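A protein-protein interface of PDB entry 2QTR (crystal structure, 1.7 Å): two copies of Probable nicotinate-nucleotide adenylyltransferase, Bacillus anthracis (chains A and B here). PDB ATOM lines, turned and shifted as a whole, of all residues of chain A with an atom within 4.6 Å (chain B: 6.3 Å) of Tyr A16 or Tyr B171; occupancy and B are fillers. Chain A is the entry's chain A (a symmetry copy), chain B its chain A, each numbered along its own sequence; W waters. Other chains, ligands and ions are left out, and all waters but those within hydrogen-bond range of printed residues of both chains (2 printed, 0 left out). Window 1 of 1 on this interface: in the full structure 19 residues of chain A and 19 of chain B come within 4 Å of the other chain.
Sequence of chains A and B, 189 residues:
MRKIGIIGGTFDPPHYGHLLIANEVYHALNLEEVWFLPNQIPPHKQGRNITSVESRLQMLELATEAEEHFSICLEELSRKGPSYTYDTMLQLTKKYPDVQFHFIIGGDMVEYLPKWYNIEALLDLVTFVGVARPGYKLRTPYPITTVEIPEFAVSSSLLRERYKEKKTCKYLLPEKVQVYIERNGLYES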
ATOM      1  N   HIS A  15     -24.052  -5.336  10.180  1.00  0.00           N
ATOM      2  CA  HIS A  15     -24.476  -5.814   8.869  1.00  0.00           C
ATOM      3  C   HIS A  15     -24.914  -4.657   7.973  1.00  0.00           C
ATOM      4  O   HIS A  15     -24.784  -3.491   8.359  1.00  0.00           O
ATOM      5  CB  HIS A  15     -25.614  -6.844   9.002  1.00  0.00           C
ATOM      6  CG  HIS A  15     -26.748  -6.390   9.864  1.00  0.00           C
ATOM      7  ND1 HIS A  15     -27.462  -5.238   9.607  1.00  0.00           N
ATOM      8  CD2 HIS A  15     -27.290  -6.928  10.986  1.00  0.00           C
ATOM      9  CE1 HIS A  15     -28.393  -5.084  10.536  1.00  0.00           C
ATOM     10  NE2 HIS A  15     -28.309  -6.096  11.386  1.00  0.00           N
ATOM     11  N   TYR A  16     -25.426  -4.980   6.790  1.00  0.00           N
ATOM     12  CA  TYR A  16     -25.826  -3.924   5.866  1.00  0.00           C
ATOM     13  C   TYR A  16     -26.981  -3.055   6.337  1.00  0.00           C
ATOM     14  O   TYR A  16     -27.143  -1.935   5.840  1.00  0.00           O
ATOM     15  CB  TYR A  16     -26.086  -4.499   4.470  1.00  0.00           C
ATOM     16  CG  TYR A  16     -24.814  -4.613   3.666  1.00  0.00           C
ATOM     17  CD1 TYR A  16     -24.415  -5.830   3.117  1.00  0.00           C
ATOM     18  CD2 TYR A  16     -23.988  -3.509   3.484  1.00  0.00           C
ATOM     19  CE1 TYR A  16     -23.217  -5.942   2.408  1.00  0.00           C
ATOM     20  CE2 TYR A  16     -22.787  -3.615   2.780  1.00  0.00           C
ATOM     21  CZ  TYR A  16     -22.411  -4.835   2.249  1.00  0.00           C
ATOM     22  OH  TYR A  16     -21.204  -4.953   1.580  1.00  0.00           O
ATOM     23  N   GLY A  17     -27.770  -3.547   7.293  1.00  0.00           N
ATOM     24  CA  GLY A  17     -28.855  -2.737   7.818  1.00  0.00           C
ATOM     25  C   GLY A  17     -28.282  -1.534   8.536  1.00  0.00           C
ATOM     26  O   GLY A  17     -28.778  -0.419   8.389  1.00  0.00           O
ATOM     27  N   HIS A  18     -27.213  -1.744   9.310  1.00  0.00           N
ATOM     28  CA  HIS A  18     -26.587  -0.657  10.045  1.00  0.00           C
ATOM     29  C   HIS A  18     -26.002   0.383   9.097  1.00  0.00           C
ATOM     30  O   HIS A  18     -26.142   1.587   9.325  1.00  0.00           O
ATOM     31  CB  HIS A  18     -25.460  -1.182  10.961  1.00  0.00           C
ATOM     32  CG  HIS A  18     -25.914  -2.206  11.956  1.00  0.00           C
ATOM     33  ND1 HIS A  18     -25.456  -3.508  11.951  1.00  0.00           N
ATOM     34  CD2 HIS A  18     -26.847  -2.139  12.941  1.00  0.00           C
ATOM     35  CE1 HIS A  18     -26.096  -4.199  12.880  1.00  0.00           C
ATOM     36  NE2 HIS A  18     -26.945  -3.393  13.494  1.00  0.00           N
ATOM     37  N   LEU A  19     -25.309  -0.095   8.074  1.00  0.00           N
ATOM     38  CA  LEU A  19     -24.671   0.778   7.091  1.00  0.00           C
ATOM     39  C   LEU A  19     -25.717   1.526   6.271  1.00  0.00           C
ATOM     40  O   LEU A  19     -25.558   2.714   5.968  1.00  0.00           O
ATOM     41  CB  LEU A  19     -23.776  -0.055   6.161  1.00  0.00           C
ATOM     42  CG  LEU A  19     -22.307  -0.285   6.563  1.00  0.00           C
ATOM     43  CD1 LEU A  19     -22.135  -0.201   8.057  1.00  0.00           C
ATOM     44  CD2 LEU A  19     -21.843  -1.629   6.008  1.00  0.00           C
ATOM     45  N   LEU A  20     -26.787   0.821   5.923  1.00  0.00           N
ATOM     46  CA  LEU A  20     -27.874   1.400   5.137  1.00  0.00           C
ATOM     47  C   LEU A  20     -28.505   2.583   5.883  1.00  0.00           C
ATOM     48  O   LEU A  20     -28.536   3.700   5.368  1.00  0.00           O
ATOM     49  CB  LEU A  20     -28.935   0.327   4.853  1.00  0.00           C
ATOM     50  CG  LEU A  20     -29.904   0.487   3.671  1.00  0.00           C
ATOM     51  CD1 LEU A  20     -31.115  -0.423   3.892  1.00  0.00           C
ATOM     52  CD2 LEU A  20     -30.351   1.925   3.552  1.00  0.00           C
ATOM     53  N   ASN A  23     -26.161   5.579   6.245  1.00  0.00           N
ATOM     54  CA  ASN A  23     -26.003   6.348   5.003  1.00  0.00           C
ATOM     55  C   ASN A  23     -27.261   7.158   4.685  1.00  0.00           C
ATOM     56  O   ASN A  23     -27.173   8.353   4.392  1.00  0.00           O
ATOM     57  CB  ASN A  23     -25.697   5.423   3.820  1.00  0.00           C
ATOM     58  CG  ASN A  23     -25.413   6.200   2.536  1.00  0.00           C
ATOM     59  OD1 ASN A  23     -24.458   6.975   2.466  1.00  0.00           O
ATOM     60  ND2 ASN A  23     -26.247   6.005   1.531  1.00  0.00           N
ATOM     61  N   GLU A  67     -15.510   3.638   4.518  1.00  0.00           N
ATOM     62  CA  GLU A  67     -16.631   4.571   4.487  1.00  0.00           C
ATOM     63  C   GLU A  67     -16.160   5.843   5.176  1.00  0.00           C
ATOM     64  O   GLU A  67     -16.142   5.921   6.395  1.00  0.00           O
ATOM     65  CB  GLU A  67     -17.830   3.966   5.217  1.00  0.00           C
ATOM     66  CG  GLU A  67     -18.158   2.526   4.792  1.00  0.00           C
ATOM     67  CD  GLU A  67     -18.637   2.415   3.346  1.00  0.00           C
ATOM     68  OE1 GLU A  67     -17.999   3.009   2.448  1.00  0.00           O
ATOM     69  OE2 GLU A  67     -19.648   1.719   3.103  1.00  0.00           O
ATOM     70  N   PHE A  70     -18.186   7.647   7.992  1.00  0.00           N
ATOM     71  CA  PHE A  70     -18.444   6.859   9.198  1.00  0.00           C
ATOM     72  C   PHE A  70     -17.211   6.745  10.075  1.00  0.00           C
ATOM     73  O   PHE A  70     -16.105   6.585   9.570  1.00  0.00           O
ATOM     74  CB  PHE A  70     -18.871   5.445   8.810  1.00  0.00           C
ATOM     75  CG  PHE A  70     -20.102   5.383   7.954  1.00  0.00           C
ATOM     76  CD1 PHE A  70     -20.382   4.241   7.228  1.00  0.00           C
ATOM     77  CD2 PHE A  70     -20.982   6.454   7.883  1.00  0.00           C
ATOM     78  CE1 PHE A  70     -21.528   4.157   6.433  1.00  0.00           C
ATOM     79  CE2 PHE A  70     -22.123   6.381   7.098  1.00  0.00           C
ATOM     80  CZ  PHE A  70     -22.397   5.230   6.373  1.00  0.00           C
ATOM     81  N   PHE A 152     -35.159  -2.893   5.266  1.00  0.00           N
ATOM     82  CA  PHE A 152     -34.387  -4.136   5.098  1.00  0.00           C
ATOM     83  C   PHE A 152     -34.515  -4.932   6.416  1.00  0.00           C
ATOM     84  O   PHE A 152     -34.024  -4.497   7.438  1.00  0.00           O
ATOM     85  CB  PHE A 152     -32.918  -3.772   4.848  1.00  0.00           C
ATOM     86  CG  PHE A 152     -32.068  -4.893   4.253  1.00  0.00           C
ATOM     87  CD1 PHE A 152     -30.712  -4.668   3.999  1.00  0.00           C
ATOM     88  CD2 PHE A 152     -32.602  -6.149   3.957  1.00  0.00           C
ATOM     89  CE1 PHE A 152     -29.896  -5.677   3.462  1.00  0.00           C
ATOM     90  CE2 PHE A 152     -31.803  -7.162   3.421  1.00  0.00           C
ATOM     91  CZ  PHE A 152     -30.442  -6.931   3.173  1.00  0.00           C
ATOM     92  N   TYR A 171     -25.256 -10.930   0.595  1.00  0.00           N
ATOM     93  CA  TYR A 171     -25.922  -9.636   0.502  1.00  0.00           C
ATOM     94  C   TYR A 171     -26.328  -9.037   1.841  1.00  0.00           C
ATOM     95  O   TYR A 171     -26.702  -7.857   1.904  1.00  0.00           O
ATOM     96  CB  TYR A 171     -27.169  -9.746  -0.393  1.00  0.00           C
ATOM     97  CG  TYR A 171     -26.912 -10.329  -1.769  1.00  0.00           C
ATOM     98  CD1 TYR A 171     -27.689 -11.371  -2.260  1.00  0.00           C
ATOM     99  CD2 TYR A 171     -25.911  -9.817  -2.588  1.00  0.00           C
ATOM    100  CE1 TYR A 171     -27.478 -11.890  -3.537  1.00  0.00           C
ATOM    101  CE2 TYR A 171     -25.694 -10.324  -3.870  1.00  0.00           C
ATOM    102  CZ  TYR A 171     -26.482 -11.360  -4.334  1.00  0.00           C
ATOM    103  OH  TYR A 171     -26.290 -11.863  -5.593  1.00  0.00           O
ATOM    104  N   LEU A 172     -26.223  -9.819   2.921  1.00  0.00           N
ATOM    105  CA  LEU A 172     -26.669  -9.331   4.223  1.00  0.00           C
ATOM    106  C   LEU A 172     -25.684  -8.537   5.088  1.00  0.00           C
ATOM    107  O   LEU A 172     -26.112  -7.750   5.931  1.00  0.00           O
ATOM    108  CB  LEU A 172     -27.244 -10.499   5.033  1.00  0.00           C
ATOM    109  CG  LEU A 172     -28.171 -11.464   4.309  1.00  0.00           C
ATOM    110  CD1 LEU A 172     -28.741 -12.448   5.337  1.00  0.00           C
ATOM    111  CD2 LEU A 172     -29.322 -10.701   3.627  1.00  0.00           C
ATOM    112  N   LEU A 173     -24.376  -8.740   4.896  1.00  0.00           N
ATOM    113  CA  LEU A 173     -23.363  -8.002   5.660  1.00  0.00           C
ATOM    114  C   LEU A 173     -22.085  -7.948   4.813  1.00  0.00           C
ATOM    115  O   LEU A 173     -21.905  -8.772   3.932  1.00  0.00           O
ATOM    116  CB  LEU A 173     -23.085  -8.692   7.012  1.00  0.00           C
ATOM    117  CG  LEU A 173     -22.342 -10.033   7.006  1.00  0.00           C
ATOM    118  CD1 LEU A 173     -22.046 -10.435   8.441  1.00  0.00           C
ATOM    119  CD2 LEU A 173     -23.150 -11.105   6.302  1.00  0.00           C
ATOM    120  N   PRO A 174     -21.185  -6.985   5.080  1.00  0.00           N
ATOM    121  CA  PRO A 174     -19.949  -6.880   4.287  1.00  0.00           C
ATOM    122  C   PRO A 174     -19.102  -8.142   4.208  1.00  0.00           C
ATOM    123  O   PRO A 174     -18.995  -8.911   5.162  1.00  0.00           O
ATOM    124  CB  PRO A 174     -19.205  -5.725   4.953  1.00  0.00           C
ATOM    125  CG  PRO A 174     -20.326  -4.875   5.516  1.00  0.00           C
ATOM    126  CD  PRO A 174     -21.230  -5.929   6.101  1.00  0.00           C
ATOM    127  N   GLU A 175     -18.508  -8.340   3.041  1.00  0.00           N
ATOM    128  CA  GLU A 175     -17.656  -9.483   2.777  1.00  0.00           C
ATOM    129  C   GLU A 175     -16.535  -9.663   3.806  1.00  0.00           C
ATOM    130  O   GLU A 175     -16.251 -10.786   4.219  1.00  0.00           O
ATOM    131  CB  GLU A 175     -17.049  -9.327   1.383  1.00  0.00           C
ATOM    132  CG  GLU A 175     -15.912 -10.280   1.069  1.00  0.00           C
ATOM    133  CD  GLU A 175     -16.348 -11.729   1.031  1.00  0.00           C
ATOM    134  OE1 GLU A 175     -17.566 -11.988   0.875  1.00  0.00           O
ATOM    135  OE2 GLU A 175     -15.464 -12.608   1.142  1.00  0.00           O
ATOM    136  N   TYR B  16     -30.427  -4.770  -5.803  1.00  0.00           N
ATOM    137  CA  TYR B  16     -30.159  -5.819  -4.826  1.00  0.00           C
ATOM    138  C   TYR B  16     -31.382  -6.589  -4.352  1.00  0.00           C
ATOM    139  O   TYR B  16     -31.239  -7.707  -3.846  1.00  0.00           O
ATOM    140  CB  TYR B  16     -29.348  -5.268  -3.650  1.00  0.00           C
ATOM    141  CG  TYR B  16     -27.868  -5.269  -3.941  1.00  0.00           C
ATOM    142  CD1 TYR B  16     -27.114  -4.101  -3.851  1.00  0.00           C
ATOM    143  CD2 TYR B  16     -27.225  -6.436  -4.343  1.00  0.00           C
ATOM    144  CE1 TYR B  16     -25.753  -4.097  -4.159  1.00  0.00           C
ATOM    145  CE2 TYR B  16     -25.865  -6.437  -4.658  1.00  0.00           C
ATOM    146  CZ  TYR B  16     -25.140  -5.263  -4.565  1.00  0.00           C
ATOM    147  OH  TYR B  16     -23.798  -5.253  -4.910  1.00  0.00           O
ATOM    148  N   PHE B 152     -36.580  -6.187   2.041  1.00  0.00           N
ATOM    149  CA  PHE B 152     -35.816  -5.010   1.598  1.00  0.00           C
ATOM    150  C   PHE B 152     -36.755  -4.169   0.705  1.00  0.00           C
ATOM    151  O   PHE B 152     -37.132  -4.609  -0.363  1.00  0.00           O
ATOM    152  CB  PHE B 152     -34.608  -5.486   0.783  1.00  0.00           C
ATOM    153  CG  PHE B 152     -33.502  -4.448   0.601  1.00  0.00           C
ATOM    154  CD1 PHE B 152     -32.363  -4.777  -0.138  1.00  0.00           C
ATOM    155  CD2 PHE B 152     -33.595  -3.165   1.146  1.00  0.00           C
ATOM    156  CE1 PHE B 152     -31.330  -3.846  -0.337  1.00  0.00           C
ATOM    157  CE2 PHE B 152     -32.576  -2.229   0.957  1.00  0.00           C
ATOM    158  CZ  PHE B 152     -31.437  -2.565   0.211  1.00  0.00           C
ATOM    159  N   CYS B 169     -27.786   6.227  -3.757  1.00  0.00           N
ATOM    160  CA  CYS B 169     -28.233   4.909  -4.156  1.00  0.00           C
ATOM    161  C   CYS B 169     -27.283   3.850  -3.597  1.00  0.00           C
ATOM    162  O   CYS B 169     -27.340   2.692  -3.991  1.00  0.00           O
ATOM    163  CB  CYS B 169     -28.307   4.822  -5.685  1.00  0.00           C
ATOM    164  SG  CYS B 169     -29.537   5.977  -6.391  1.00  0.00           S
ATOM    165  N   LYS B 170     -26.427   4.263  -2.666  1.00  0.00           N
ATOM    166  CA  LYS B 170     -25.465   3.352  -2.041  1.00  0.00           C
ATOM    167  C   LYS B 170     -26.168   2.167  -1.374  1.00  0.00           C
ATOM    168  O   LYS B 170     -27.181   2.340  -0.701  1.00  0.00           O
ATOM    169  CB  LYS B 170     -24.639   4.113  -1.007  1.00  0.00           C
ATOM    170  CG  LYS B 170     -23.401   3.373  -0.497  1.00  0.00           C
ATOM    171  CD  LYS B 170     -22.536   4.304   0.349  1.00  0.00           C
ATOM    172  CE  LYS B 170     -21.228   3.652   0.743  1.00  0.00           C
ATOM    173  NZ  LYS B 170     -20.420   4.542   1.631  1.00  0.00           N
ATOM    174  N   TYR B 171     -25.623   0.972  -1.587  1.00  0.00           N
ATOM    175  CA  TYR B 171     -26.136  -0.273  -1.025  1.00  0.00           C
ATOM    176  C   TYR B 171     -27.392  -0.802  -1.703  1.00  0.00           C
ATOM    177  O   TYR B 171     -27.791  -1.949  -1.458  1.00  0.00           O
ATOM    178  CB  TYR B 171     -26.417  -0.099   0.478  1.00  0.00           C
ATOM    179  CG  TYR B 171     -25.244   0.425   1.286  1.00  0.00           C
ATOM    180  CD1 TYR B 171     -25.395   1.506   2.145  1.00  0.00           C
ATOM    181  CD2 TYR B 171     -23.995  -0.183   1.209  1.00  0.00           C
ATOM    182  CE1 TYR B 171     -24.329   1.971   2.914  1.00  0.00           C
ATOM    183  CE2 TYR B 171     -22.922   0.270   1.977  1.00  0.00           C
ATOM    184  CZ  TYR B 171     -23.099   1.347   2.826  1.00  0.00           C
ATOM    185  OH  TYR B 171     -22.060   1.798   3.595  1.00  0.00           O
ATOM    186  N   LEU B 172     -28.000   0.001  -2.582  1.00  0.00           N
ATOM    187  CA  LEU B 172     -29.251  -0.416  -3.209  1.00  0.00           C
ATOM    188  C   LEU B 172     -29.189  -1.254  -4.491  1.00  0.00           C
ATOM    189  O   LEU B 172     -30.133  -1.983  -4.788  1.00  0.00           O
ATOM    190  CB  LEU B 172     -30.138   0.814  -3.437  1.00  0.00           C
ATOM    191  CG  LEU B 172     -30.243   1.823  -2.303  1.00  0.00           C
ATOM    192  CD1 LEU B 172     -31.289   2.875  -2.688  1.00  0.00           C
ATOM    193  CD2 LEU B 172     -30.663   1.126  -0.996  1.00  0.00           C
ATOM    194  N   LEU B 173     -28.095  -1.152  -5.254  1.00  0.00           N
ATOM    195  CA  LEU B 173     -27.939  -1.938  -6.484  1.00  0.00           C
ATOM    196  C   LEU B 173     -26.437  -2.109  -6.743  1.00  0.00           C
ATOM    197  O   LEU B 173     -25.642  -1.326  -6.249  1.00  0.00           O
ATOM    198  CB  LEU B 173     -28.615  -1.232  -7.677  1.00  0.00           C
ATOM    199  CG  LEU B 173     -27.976   0.051  -8.221  1.00  0.00           C
ATOM    200  CD1 LEU B 173     -28.716   0.471  -9.479  1.00  0.00           C
ATOM    201  CD2 LEU B 173     -28.000   1.158  -7.186  1.00  0.00           C
ATOM    202  N   GLN B 178     -24.574   0.755 -11.313  1.00  0.00           N
ATOM    203  CA  GLN B 178     -24.543   2.181 -11.021  1.00  0.00           C
ATOM    204  C   GLN B 178     -23.650   2.887 -12.052  1.00  0.00           C
ATOM    205  O   GLN B 178     -24.001   3.945 -12.573  1.00  0.00           O
ATOM    206  CB  GLN B 178     -23.998   2.427  -9.605  1.00  0.00           C
ATOM    207  CG  GLN B 178     -24.914   1.926  -8.473  1.00  0.00           C
ATOM    208  CD  GLN B 178     -24.340   2.169  -7.083  1.00  0.00           C
ATOM    209  OE1 GLN B 178     -24.032   3.302  -6.715  1.00  0.00           O
ATOM    210  NE2 GLN B 178     -24.201   1.099  -6.301  1.00  0.00           N
HETATM  211  O   HOH W   1     -27.215  -4.904   0.210  1.00  0.00           O
HETATM  212  O   HOH W   2     -28.259   4.218   1.215  1.00  0.00           O
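O of Leu B172 lies within hydrogen-bond range of N of Tyr B16, at 3.0 Å. The backbone NH (N) of Tyr A16 sits at hydrogen-bond distance from the backbone carbonyl oxygen (O) of Leu A172.
Tyr A16 touches Tyr B171, and with the chains exchanged Tyr A171 touches Tyr B16. Phe A152 touches its own counterpart, Phe B152. Positions printed for both chains: 16, 152, 171, 172 and 173. Of the 11 pairs that touch across the chains among the printed residues, 3 have their exchanged pair printed and touching as well.
The side-chain carboxylate of Glu A67 lies within salt-bridge range of the side-chain amino group of Lys B170 (3.0 Å). OH of Tyr B171 lies within hydrogen-bond range of OE2 of Glu A67 (2.5 Å).
Of the printed residues of chain B, Leu A19 touches Tyr B171 (3.4 Å). Of the printed residues of chain B, Leu A20 touches Phe B152 and Tyr B171. Printed residues of chain B within 4 Å of Phe A70: Tyr B171 (3.7 Å). Of the printed residues of chain B, Phe A152 touches Phe B152. Leu A173 touches none of the printed residues of chain B. Glu A175 touches none of the printed residues of chain B. Of the printed residues of chain A, Tyr B171 touches Tyr A16, Leu A19, Leu A20, Asn A23, Glu A67 and Phe A70. The nearest printed residue of chain B that does not touch Tyr A16 is Tyr B16 (7.0 Å). The nearest printed residue of chain B that does not touch Tyr A171 is Phe B152 (6.5 Å).
Among the printed residues, merely in contact across the chains: Tyr A16 with Tyr B171 (3.96 Å), Leu A19 with Tyr B171 (3.4 Å), Leu A20 with Phe B152 (3.7 Å), Leu A20 with Tyr B171 (3.9 Å), Asn A23 with Lys B170 (3.6 Å), Asn A23 with Tyr B171 (3.8 Å), Phe A70 with Tyr B171 (3.7 Å), Phe A152 with Phe B152 (3.8 Å) and Tyr A171 with Tyr B16 (3.96 Å).
Printed residues of chain A that touch a printed residue of chain B: Tyr A16, Leu A19, Leu A20, Asn A23, Glu A67, Phe A70, Phe A152 and Tyr A171. Hydrophobic or aromatic side chains of chain A within 4 Å of the printed part of chain B: Tyr A16, Leu A19, Leu A20, Phe A70, Phe A152 and Tyr A171. Along chain A the printed residues that touch a printed residue of chain B span positions 16 to 171. Of the 8 printed residues of chain B, 4 touch a printed residue of chain A. Hydrophobic or aromatic side chains of chain B that line the printed part of chain A: Tyr B16, Phe B152 and Tyr B171. Among the printed residues, 11 pairs touch across the chains. Among the printed residues, Asp or Glu carboxylates within 4 Å of a Lys or Arg side-chain nitrogen of the other chain: Glu A67 with Lys B170 (3.0 Å).
Water W2 lies within hydrogen-bond range of ND2 of Asn A23 and O of Lys B170. Water W1 bridges the backbone carbonyl oxygen (O) of Tyr B171 (3.4 Å) and the backbone carbonyl oxygen (O) of Tyr A171 (3.4 Å).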
